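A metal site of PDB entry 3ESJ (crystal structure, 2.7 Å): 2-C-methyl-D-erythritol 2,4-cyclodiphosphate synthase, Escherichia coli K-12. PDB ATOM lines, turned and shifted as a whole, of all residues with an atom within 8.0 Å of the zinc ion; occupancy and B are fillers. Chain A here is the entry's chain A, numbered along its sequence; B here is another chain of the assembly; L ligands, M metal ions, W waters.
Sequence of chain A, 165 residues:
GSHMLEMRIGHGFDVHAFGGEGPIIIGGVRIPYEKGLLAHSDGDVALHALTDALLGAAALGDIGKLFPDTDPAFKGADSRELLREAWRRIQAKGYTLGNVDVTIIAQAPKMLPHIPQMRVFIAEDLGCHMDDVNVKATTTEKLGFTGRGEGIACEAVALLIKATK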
ATOM      1  N   PHE A  13      24.455 -20.784  -9.446  1.00  0.00           N
ATOM      2  CA  PHE A  13      23.155 -21.229  -9.950  1.00  0.00           C
ATOM      3  C   PHE A  13      22.861 -22.680  -9.483  1.00  0.00           C
ATOM      4  O   PHE A  13      23.760 -23.530  -9.497  1.00  0.00           O
ATOM      5  CB  PHE A  13      23.114 -21.092 -11.469  1.00  0.00           C
ATOM      6  CG  PHE A  13      21.905 -21.695 -12.086  1.00  0.00           C
ATOM      7  CD1 PHE A  13      20.737 -20.967 -12.214  1.00  0.00           C
ATOM      8  CD2 PHE A  13      21.921 -23.019 -12.529  1.00  0.00           C
ATOM      9  CE1 PHE A  13      19.606 -21.539 -12.771  1.00  0.00           C
ATOM     10  CE2 PHE A  13      20.780 -23.602 -13.110  1.00  0.00           C
ATOM     11  CZ  PHE A  13      19.627 -22.856 -13.219  1.00  0.00           C
ATOM     12  N   ASP A  14      21.631 -22.936  -9.039  1.00  0.00           N
ATOM     13  CA  ASP A  14      21.280 -24.280  -8.577  1.00  0.00           C
ATOM     14  C   ASP A  14      19.836 -24.661  -8.911  1.00  0.00           C
ATOM     15  O   ASP A  14      18.967 -23.778  -9.068  1.00  0.00           O
ATOM     16  CB  ASP A  14      21.540 -24.405  -7.078  1.00  0.00           C
ATOM     17  CG  ASP A  14      21.468 -25.832  -6.579  1.00  0.00           C
ATOM     18  OD1 ASP A  14      21.615 -26.748  -7.407  1.00  0.00           O
ATOM     19  OD2 ASP A  14      21.245 -26.046  -5.367  1.00  0.00           O
ATOM     20  N   VAL A  15      19.583 -25.961  -9.041  1.00  0.00           N
ATOM     21  CA  VAL A  15      18.248 -26.480  -9.279  1.00  0.00           C
ATOM     22  C   VAL A  15      18.006 -27.712  -8.405  1.00  0.00           C
ATOM     23  O   VAL A  15      18.902 -28.523  -8.226  1.00  0.00           O
ATOM     24  CB  VAL A  15      18.051 -26.876 -10.773  1.00  0.00           C
ATOM     25  CG1 VAL A  15      16.714 -27.600 -10.959  1.00  0.00           C
ATOM     26  CG2 VAL A  15      18.117 -25.647 -11.683  1.00  0.00           C
ATOM     27  N   HIS A  16      16.794 -27.848  -7.872  1.00  0.00           N
ATOM     28  CA  HIS A  16      16.334 -29.118  -7.286  1.00  0.00           C
ATOM     29  C   HIS A  16      14.907 -29.475  -7.722  1.00  0.00           C
ATOM     30  O   HIS A  16      14.080 -28.574  -7.947  1.00  0.00           O
ATOM     31  CB  HIS A  16      16.524 -29.142  -5.759  1.00  0.00           C
ATOM     32  CG  HIS A  16      17.959 -29.199  -5.341  1.00  0.00           C
ATOM     33  ND1 HIS A  16      18.736 -30.326  -5.494  1.00  0.00           N
ATOM     34  CD2 HIS A  16      18.785 -28.254  -4.839  1.00  0.00           C
ATOM     35  CE1 HIS A  16      19.965 -30.093  -5.072  1.00  0.00           C
ATOM     36  NE2 HIS A  16      20.028 -28.827  -4.673  1.00  0.00           N
ATOM     37  N   LEU A  38      13.821 -32.804  -3.578  1.00  0.00           N
ATOM     38  CA  LEU A  38      14.732 -33.933  -3.689  1.00  0.00           C
ATOM     39  C   LEU A  38      16.190 -33.476  -3.715  1.00  0.00           C
ATOM     40  O   LEU A  38      16.586 -32.696  -4.580  1.00  0.00           O
ATOM     41  CB  LEU A  38      14.429 -34.756  -4.943  1.00  0.00           C
ATOM     42  CG  LEU A  38      13.096 -35.506  -4.951  1.00  0.00           C
ATOM     43  CD1 LEU A  38      12.991 -36.417  -6.162  1.00  0.00           C
ATOM     44  CD2 LEU A  38      12.919 -36.307  -3.664  1.00  0.00           C
ATOM     45  N   ALA A  39      16.976 -33.962  -2.760  1.00  0.00           N
ATOM     46  CA  ALA A  39      18.386 -33.596  -2.664  1.00  0.00           C
ATOM     47  C   ALA A  39      19.144 -34.565  -1.773  1.00  0.00           C
ATOM     48  O   ALA A  39      18.558 -35.258  -0.945  1.00  0.00           O
ATOM     49  CB  ALA A  39      18.514 -32.170  -2.140  1.00  0.00           C
ATOM     50  N   HIS A  40      20.465 -34.612  -1.945  1.00  0.00           N
ATOM     51  CA  HIS A  40      21.345 -35.208  -0.950  1.00  0.00           C
ATOM     52  C   HIS A  40      21.299 -34.438   0.367  1.00  0.00           C
ATOM     53  O   HIS A  40      21.961 -34.819   1.339  1.00  0.00           O
ATOM     54  CB  HIS A  40      22.793 -35.254  -1.474  1.00  0.00           C
ATOM     55  CG  HIS A  40      23.715 -36.081  -0.637  1.00  0.00           C
ATOM     56  ND1 HIS A  40      25.012 -35.722  -0.386  1.00  0.00           N
ATOM     57  CD2 HIS A  40      23.513 -37.258   0.010  1.00  0.00           C
ATOM     58  CE1 HIS A  40      25.584 -36.637   0.380  1.00  0.00           C
ATOM     59  NE2 HIS A  40      24.692 -37.577   0.636  1.00  0.00           N
ATOM     60  N   SER A  41      20.508 -33.372   0.395  1.00  0.00           N
ATOM     61  CA  SER A  41      20.774 -32.243   1.268  1.00  0.00           C
ATOM     62  C   SER A  41      19.514 -31.688   1.922  1.00  0.00           C
ATOM     63  O   SER A  41      18.464 -32.324   1.894  1.00  0.00           O
ATOM     64  CB  SER A  41      21.525 -31.149   0.511  1.00  0.00           C
ATOM     65  OG  SER A  41      20.656 -30.412  -0.325  1.00  0.00           O
ATOM     66  N   ASP A  42      19.630 -30.511   2.530  1.00  0.00           N
ATOM     67  CA  ASP A  42      18.504 -29.589   2.639  1.00  0.00           C
ATOM     68  C   ASP A  42      17.676 -29.588   1.361  1.00  0.00           C
ATOM     69  O   ASP A  42      16.461 -29.374   1.393  1.00  0.00           O
ATOM     70  CB  ASP A  42      19.039 -28.185   2.923  1.00  0.00           C
ATOM     71  CG  ASP A  42      18.928 -27.801   4.385  1.00  0.00           C
ATOM     72  OD1 ASP A  42      18.515 -28.659   5.193  1.00  0.00           O
ATOM     73  OD2 ASP A  42      19.246 -26.650   4.721  1.00  0.00           O
ATOM     74  N   GLY A  43      18.327 -29.832   0.229  1.00  0.00           N
ATOM     75  CA  GLY A  43      17.834 -29.374  -1.055  1.00  0.00           C
ATOM     76  C   GLY A  43      17.698 -27.879  -1.222  1.00  0.00           C
ATOM     77  O   GLY A  43      17.133 -27.409  -2.211  1.00  0.00           O
ATOM     78  N   ASP A  44      18.207 -27.119  -0.260  1.00  0.00           N
ATOM     79  CA  ASP A  44      17.979 -25.684  -0.182  1.00  0.00           C
ATOM     80  C   ASP A  44      18.701 -25.014  -1.346  1.00  0.00           C
ATOM     81  O   ASP A  44      19.896 -24.696  -1.249  1.00  0.00           O
ATOM     82  CB  ASP A  44      18.450 -25.134   1.161  1.00  0.00           C
ATOM     83  CG  ASP A  44      18.091 -23.671   1.343  1.00  0.00           C
ATOM     84  OD1 ASP A  44      18.045 -22.941   0.338  1.00  0.00           O
ATOM     85  OD2 ASP A  44      17.862 -23.265   2.504  1.00  0.00           O
ATOM     86  N   VAL A  45      17.985 -24.781  -2.437  1.00  0.00           N
ATOM     87  CA  VAL A  45      18.582 -24.226  -3.660  1.00  0.00           C
ATOM     88  C   VAL A  45      19.075 -22.800  -3.469  1.00  0.00           C
ATOM     89  O   VAL A  45      19.997 -22.376  -4.159  1.00  0.00           O
ATOM     90  CB  VAL A  45      17.625 -24.222  -4.882  1.00  0.00           C
ATOM     91  CG1 VAL A  45      17.217 -25.578  -5.220  1.00  0.00           C
ATOM     92  CG2 VAL A  45      16.380 -23.431  -4.584  1.00  0.00           C
ATOM     93  N   ALA A  46      18.472 -22.046  -2.555  1.00  0.00           N
ATOM     94  CA  ALA A  46      18.866 -20.656  -2.378  1.00  0.00           C
ATOM     95  C   ALA A  46      20.267 -20.580  -1.761  1.00  0.00           C
ATOM     96  O   ALA A  46      21.135 -19.865  -2.273  1.00  0.00           O
ATOM     97  CB  ALA A  46      17.845 -19.865  -1.552  1.00  0.00           C
ATOM     98  N   LEU A  47      20.488 -21.329  -0.693  1.00  0.00           N
ATOM     99  CA  LEU A  47      21.778 -21.304  -0.028  1.00  0.00           C
ATOM    100  C   LEU A  47      22.869 -21.965  -0.869  1.00  0.00           C
ATOM    101  O   LEU A  47      24.040 -21.543  -0.841  1.00  0.00           O
ATOM    102  CB  LEU A  47      21.698 -21.908   1.370  1.00  0.00           C
ATOM    103  CG  LEU A  47      20.753 -21.155   2.321  1.00  0.00           C
ATOM    104  CD1 LEU A  47      20.769 -21.801   3.711  1.00  0.00           C
ATOM    105  CD2 LEU A  47      21.080 -19.666   2.417  1.00  0.00           C
ATOM    106  N   HIS A  48      22.497 -22.983  -1.643  1.00  0.00           N
ATOM    107  CA  HIS A  48      23.450 -23.602  -2.557  1.00  0.00           C
ATOM    108  C   HIS A  48      23.921 -22.603  -3.605  1.00  0.00           C
ATOM    109  O   HIS A  48      25.142 -22.433  -3.789  1.00  0.00           O
ATOM    110  CB  HIS A  48      22.889 -24.847  -3.219  1.00  0.00           C
ATOM    111  CG  HIS A  48      22.654 -25.970  -2.264  1.00  0.00           C
ATOM    112  ND1 HIS A  48      22.049 -27.151  -2.633  1.00  0.00           N
ATOM    113  CD2 HIS A  48      22.940 -26.090  -0.938  1.00  0.00           C
ATOM    114  CE1 HIS A  48      21.989 -27.949  -1.575  1.00  0.00           C
ATOM    115  NE2 HIS A  48      22.519 -27.328  -0.534  1.00  0.00           N
ATOM    116  N   ALA A  49      22.990 -21.922  -4.272  1.00  0.00           N
ATOM    117  CA  ALA A  49      23.385 -20.966  -5.300  1.00  0.00           C
ATOM    118  C   ALA A  49      24.240 -19.869  -4.662  1.00  0.00           C
ATOM    119  O   ALA A  49      25.273 -19.455  -5.214  1.00  0.00           O
ATOM    120  CB  ALA A  49      22.185 -20.413  -6.005  1.00  0.00           C
ATOM    121  N   ASP A  52      27.808 -21.110  -3.818  1.00  0.00           N
ATOM    122  CA  ASP A  52      28.600 -21.162  -5.041  1.00  0.00           C
ATOM    123  C   ASP A  52      29.049 -19.774  -5.499  1.00  0.00           C
ATOM    124  O   ASP A  52      30.175 -19.631  -5.980  1.00  0.00           O
ATOM    125  CB  ASP A  52      27.823 -21.862  -6.170  1.00  0.00           C
ATOM    126  CG  ASP A  52      28.047 -23.356  -6.210  1.00  0.00           C
ATOM    127  OD1 ASP A  52      28.790 -23.865  -5.326  1.00  0.00           O
ATOM    128  OD2 ASP A  52      27.485 -24.028  -7.121  1.00  0.00           O
ATOM    129  N   ILE A  63      30.479 -25.914  -4.243  1.00  0.00           N
ATOM    130  CA  ILE A  63      30.054 -26.871  -3.209  1.00  0.00           C
ATOM    131  C   ILE A  63      30.345 -28.317  -3.570  1.00  0.00           C
ATOM    132  O   ILE A  63      30.698 -29.090  -2.693  1.00  0.00           O
ATOM    133  CB  ILE A  63      28.568 -26.765  -2.838  1.00  0.00           C
ATOM    134  CG1 ILE A  63      27.691 -26.754  -4.099  1.00  0.00           C
ATOM    135  CG2 ILE A  63      28.298 -25.586  -1.973  1.00  0.00           C
ATOM    136  CD1 ILE A  63      26.286 -27.163  -3.868  1.00  0.00           C
ATOM    137  N   SER A  79      22.060 -26.989   5.046  1.00  0.00           N
ATOM    138  CA  SER A  79      22.780 -26.192   4.052  1.00  0.00           C
ATOM    139  C   SER A  79      23.410 -24.920   4.629  1.00  0.00           C
ATOM    140  O   SER A  79      24.339 -24.366   4.044  1.00  0.00           O
ATOM    141  CB  SER A  79      21.875 -25.846   2.862  1.00  0.00           C
ATOM    142  OG  SER A  79      21.622 -26.975   2.059  1.00  0.00           O
ATOM    143  N   LEU A  82      26.879 -25.799   5.598  1.00  0.00           N
ATOM    144  CA  LEU A  82      27.738 -25.737   4.411  1.00  0.00           C
ATOM    145  C   LEU A  82      28.117 -24.305   4.064  1.00  0.00           C
ATOM    146  O   LEU A  82      29.274 -24.021   3.783  1.00  0.00           O
ATOM    147  CB  LEU A  82      27.056 -26.403   3.216  1.00  0.00           C
ATOM    148  CG  LEU A  82      26.621 -27.858   3.421  1.00  0.00           C
ATOM    149  CD1 LEU A  82      25.758 -28.333   2.230  1.00  0.00           C
ATOM    150  CD2 LEU A  82      27.828 -28.760   3.661  1.00  0.00           C
ATOM    151  N   ILE A 152      12.556 -26.136  -8.509  1.00  0.00           N
ATOM    152  CA  ILE A 152      12.893 -24.742  -8.199  1.00  0.00           C
ATOM    153  C   ILE A 152      14.347 -24.471  -8.583  1.00  0.00           C
ATOM    154  O   ILE A 152      15.213 -25.308  -8.353  1.00  0.00           O
ATOM    155  CB  ILE A 152      12.689 -24.399  -6.676  1.00  0.00           C
ATOM    156  CG1 ILE A 152      11.218 -24.478  -6.287  1.00  0.00           C
ATOM    157  CG2 ILE A 152      13.179 -22.995  -6.347  1.00  0.00           C
ATOM    158  CD1 ILE A 152      10.940 -24.153  -4.807  1.00  0.00           C
ATOM    159  N   THR B 138      27.069 -27.089 -12.406  1.00  0.00           N
ATOM    160  CA  THR B 138      25.870 -27.598 -11.728  1.00  0.00           C
ATOM    161  C   THR B 138      25.050 -28.406 -12.713  1.00  0.00           C
ATOM    162  O   THR B 138      25.044 -28.150 -13.924  1.00  0.00           O
ATOM    163  CB  THR B 138      25.024 -26.514 -10.971  1.00  0.00           C
ATOM    164  OG1 THR B 138      23.920 -26.093 -11.752  1.00  0.00           O
ATOM    165  CG2 THR B 138      25.830 -25.286 -10.655  1.00  0.00           C
ATOM    166  N   THR B 139      24.384 -29.405 -12.164  1.00  0.00           N
ATOM    167  CA  THR B 139      23.452 -30.234 -12.896  1.00  0.00           C
ATOM    168  C   THR B 139      22.071 -29.691 -12.568  1.00  0.00           C
ATOM    169  O   THR B 139      21.907 -29.058 -11.555  1.00  0.00           O
ATOM    170  CB  THR B 139      23.583 -31.706 -12.485  1.00  0.00           C
ATOM    171  OG1 THR B 139      22.277 -32.255 -12.336  1.00  0.00           O
ATOM    172  CG2 THR B 139      24.258 -31.861 -11.118  1.00  0.00           C
ATOM    173  N   GLU B 141      19.453 -31.739 -12.200  1.00  0.00           N
ATOM    174  CA  GLU B 141      18.771 -32.894 -11.649  1.00  0.00           C
ATOM    175  C   GLU B 141      17.735 -33.477 -12.605  1.00  0.00           C
ATOM    176  O   GLU B 141      16.599 -33.745 -12.189  1.00  0.00           O
ATOM    177  CB  GLU B 141      18.085 -32.561 -10.315  1.00  0.00           C
ATOM    178  CG  GLU B 141      18.946 -31.815  -9.287  1.00  0.00           C
ATOM    179  CD  GLU B 141      20.010 -32.675  -8.642  1.00  0.00           C
ATOM    180  OE1 GLU B 141      20.410 -32.373  -7.499  1.00  0.00           O
ATOM    181  OE2 GLU B 141      20.475 -33.648  -9.286  1.00  0.00           O
HETATM  182  O1  LIG L   1      31.213 -32.043 -12.447  1.00  0.00           O
HETATM  183  C1  LIG L   1      30.063 -31.772 -12.729  1.00  0.00           C
HETATM  184  N1  LIG L   1      29.600 -31.917 -13.973  1.00  0.00           N
HETATM  185  C2  LIG L   1      28.333 -31.606 -14.271  1.00  0.00           C
HETATM  186  N2  LIG L   1      27.931 -31.758 -15.497  1.00  0.00           N
HETATM  187  C3  LIG L   1      27.448 -31.157 -13.302  1.00  0.00           C
HETATM  188  C4  LIG L   1      27.889 -31.019 -11.995  1.00  0.00           C
HETATM  189  N3  LIG L   1      29.234 -31.338 -11.721  1.00  0.00           N
HETATM  190  C5  LIG L   1      29.802 -31.228 -10.391  1.00  0.00           C
HETATM  191  O2  LIG L   1      29.380 -32.458  -9.773  1.00  0.00           O
HETATM  192  C6  LIG L   1      29.132 -32.145  -8.443  1.00  0.00           C
HETATM  193  C7  LIG L   1      28.136 -33.114  -7.826  1.00  0.00           C
HETATM  194  O3  LIG L   1      27.676 -32.599  -6.567  1.00  0.00           O
HETATM  195  P1  LIG L   1      27.153 -31.060  -6.463  1.00  0.00           P
HETATM  196  O4  LIG L   1      25.859 -30.961  -7.357  1.00  0.00           O
HETATM  197  O5  LIG L   1      27.011 -30.644  -5.051  1.00  0.00           O
HETATM  198  O6  LIG L   1      28.146 -30.241  -7.338  1.00  0.00           O
HETATM  199  C8  LIG L   1      28.353 -30.845  -8.610  1.00  0.00           C
HETATM  200  C9  LIG L   1      29.280 -30.097  -9.525  1.00  0.00           C
HETATM  201  O7  LIG L   1      30.384 -29.618  -8.771  1.00  0.00           O
HETATM  202 ZN    ZN M   1      21.761 -27.848  -4.579  1.00  0.00          ZN
HETATM  203  O   HOH W   1      23.309 -29.610  -4.752  1.00  0.00           O
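Of the 24 residues printed, 3 come within 4 Å of the zinc ion.
ND1 of His 16 lies within hydrogen-bond range of OE1 of Glu 141 of chain B. The side-chain hydroxyl of Ser 79 lies within hydrogen-bond range of a ring nitrogen (NE2) of His 48 (2.8 Å). O of His 16 sits at hydrogen-bond distance from N of Ile 152. O of Leu 38 sits at hydrogen-bond distance from ND1 of His 16, at 3.3 Å.
The zinc ion is bound by NE2 of His 16, OD2 of Asp 14, ND1 of His 48 and water W1.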
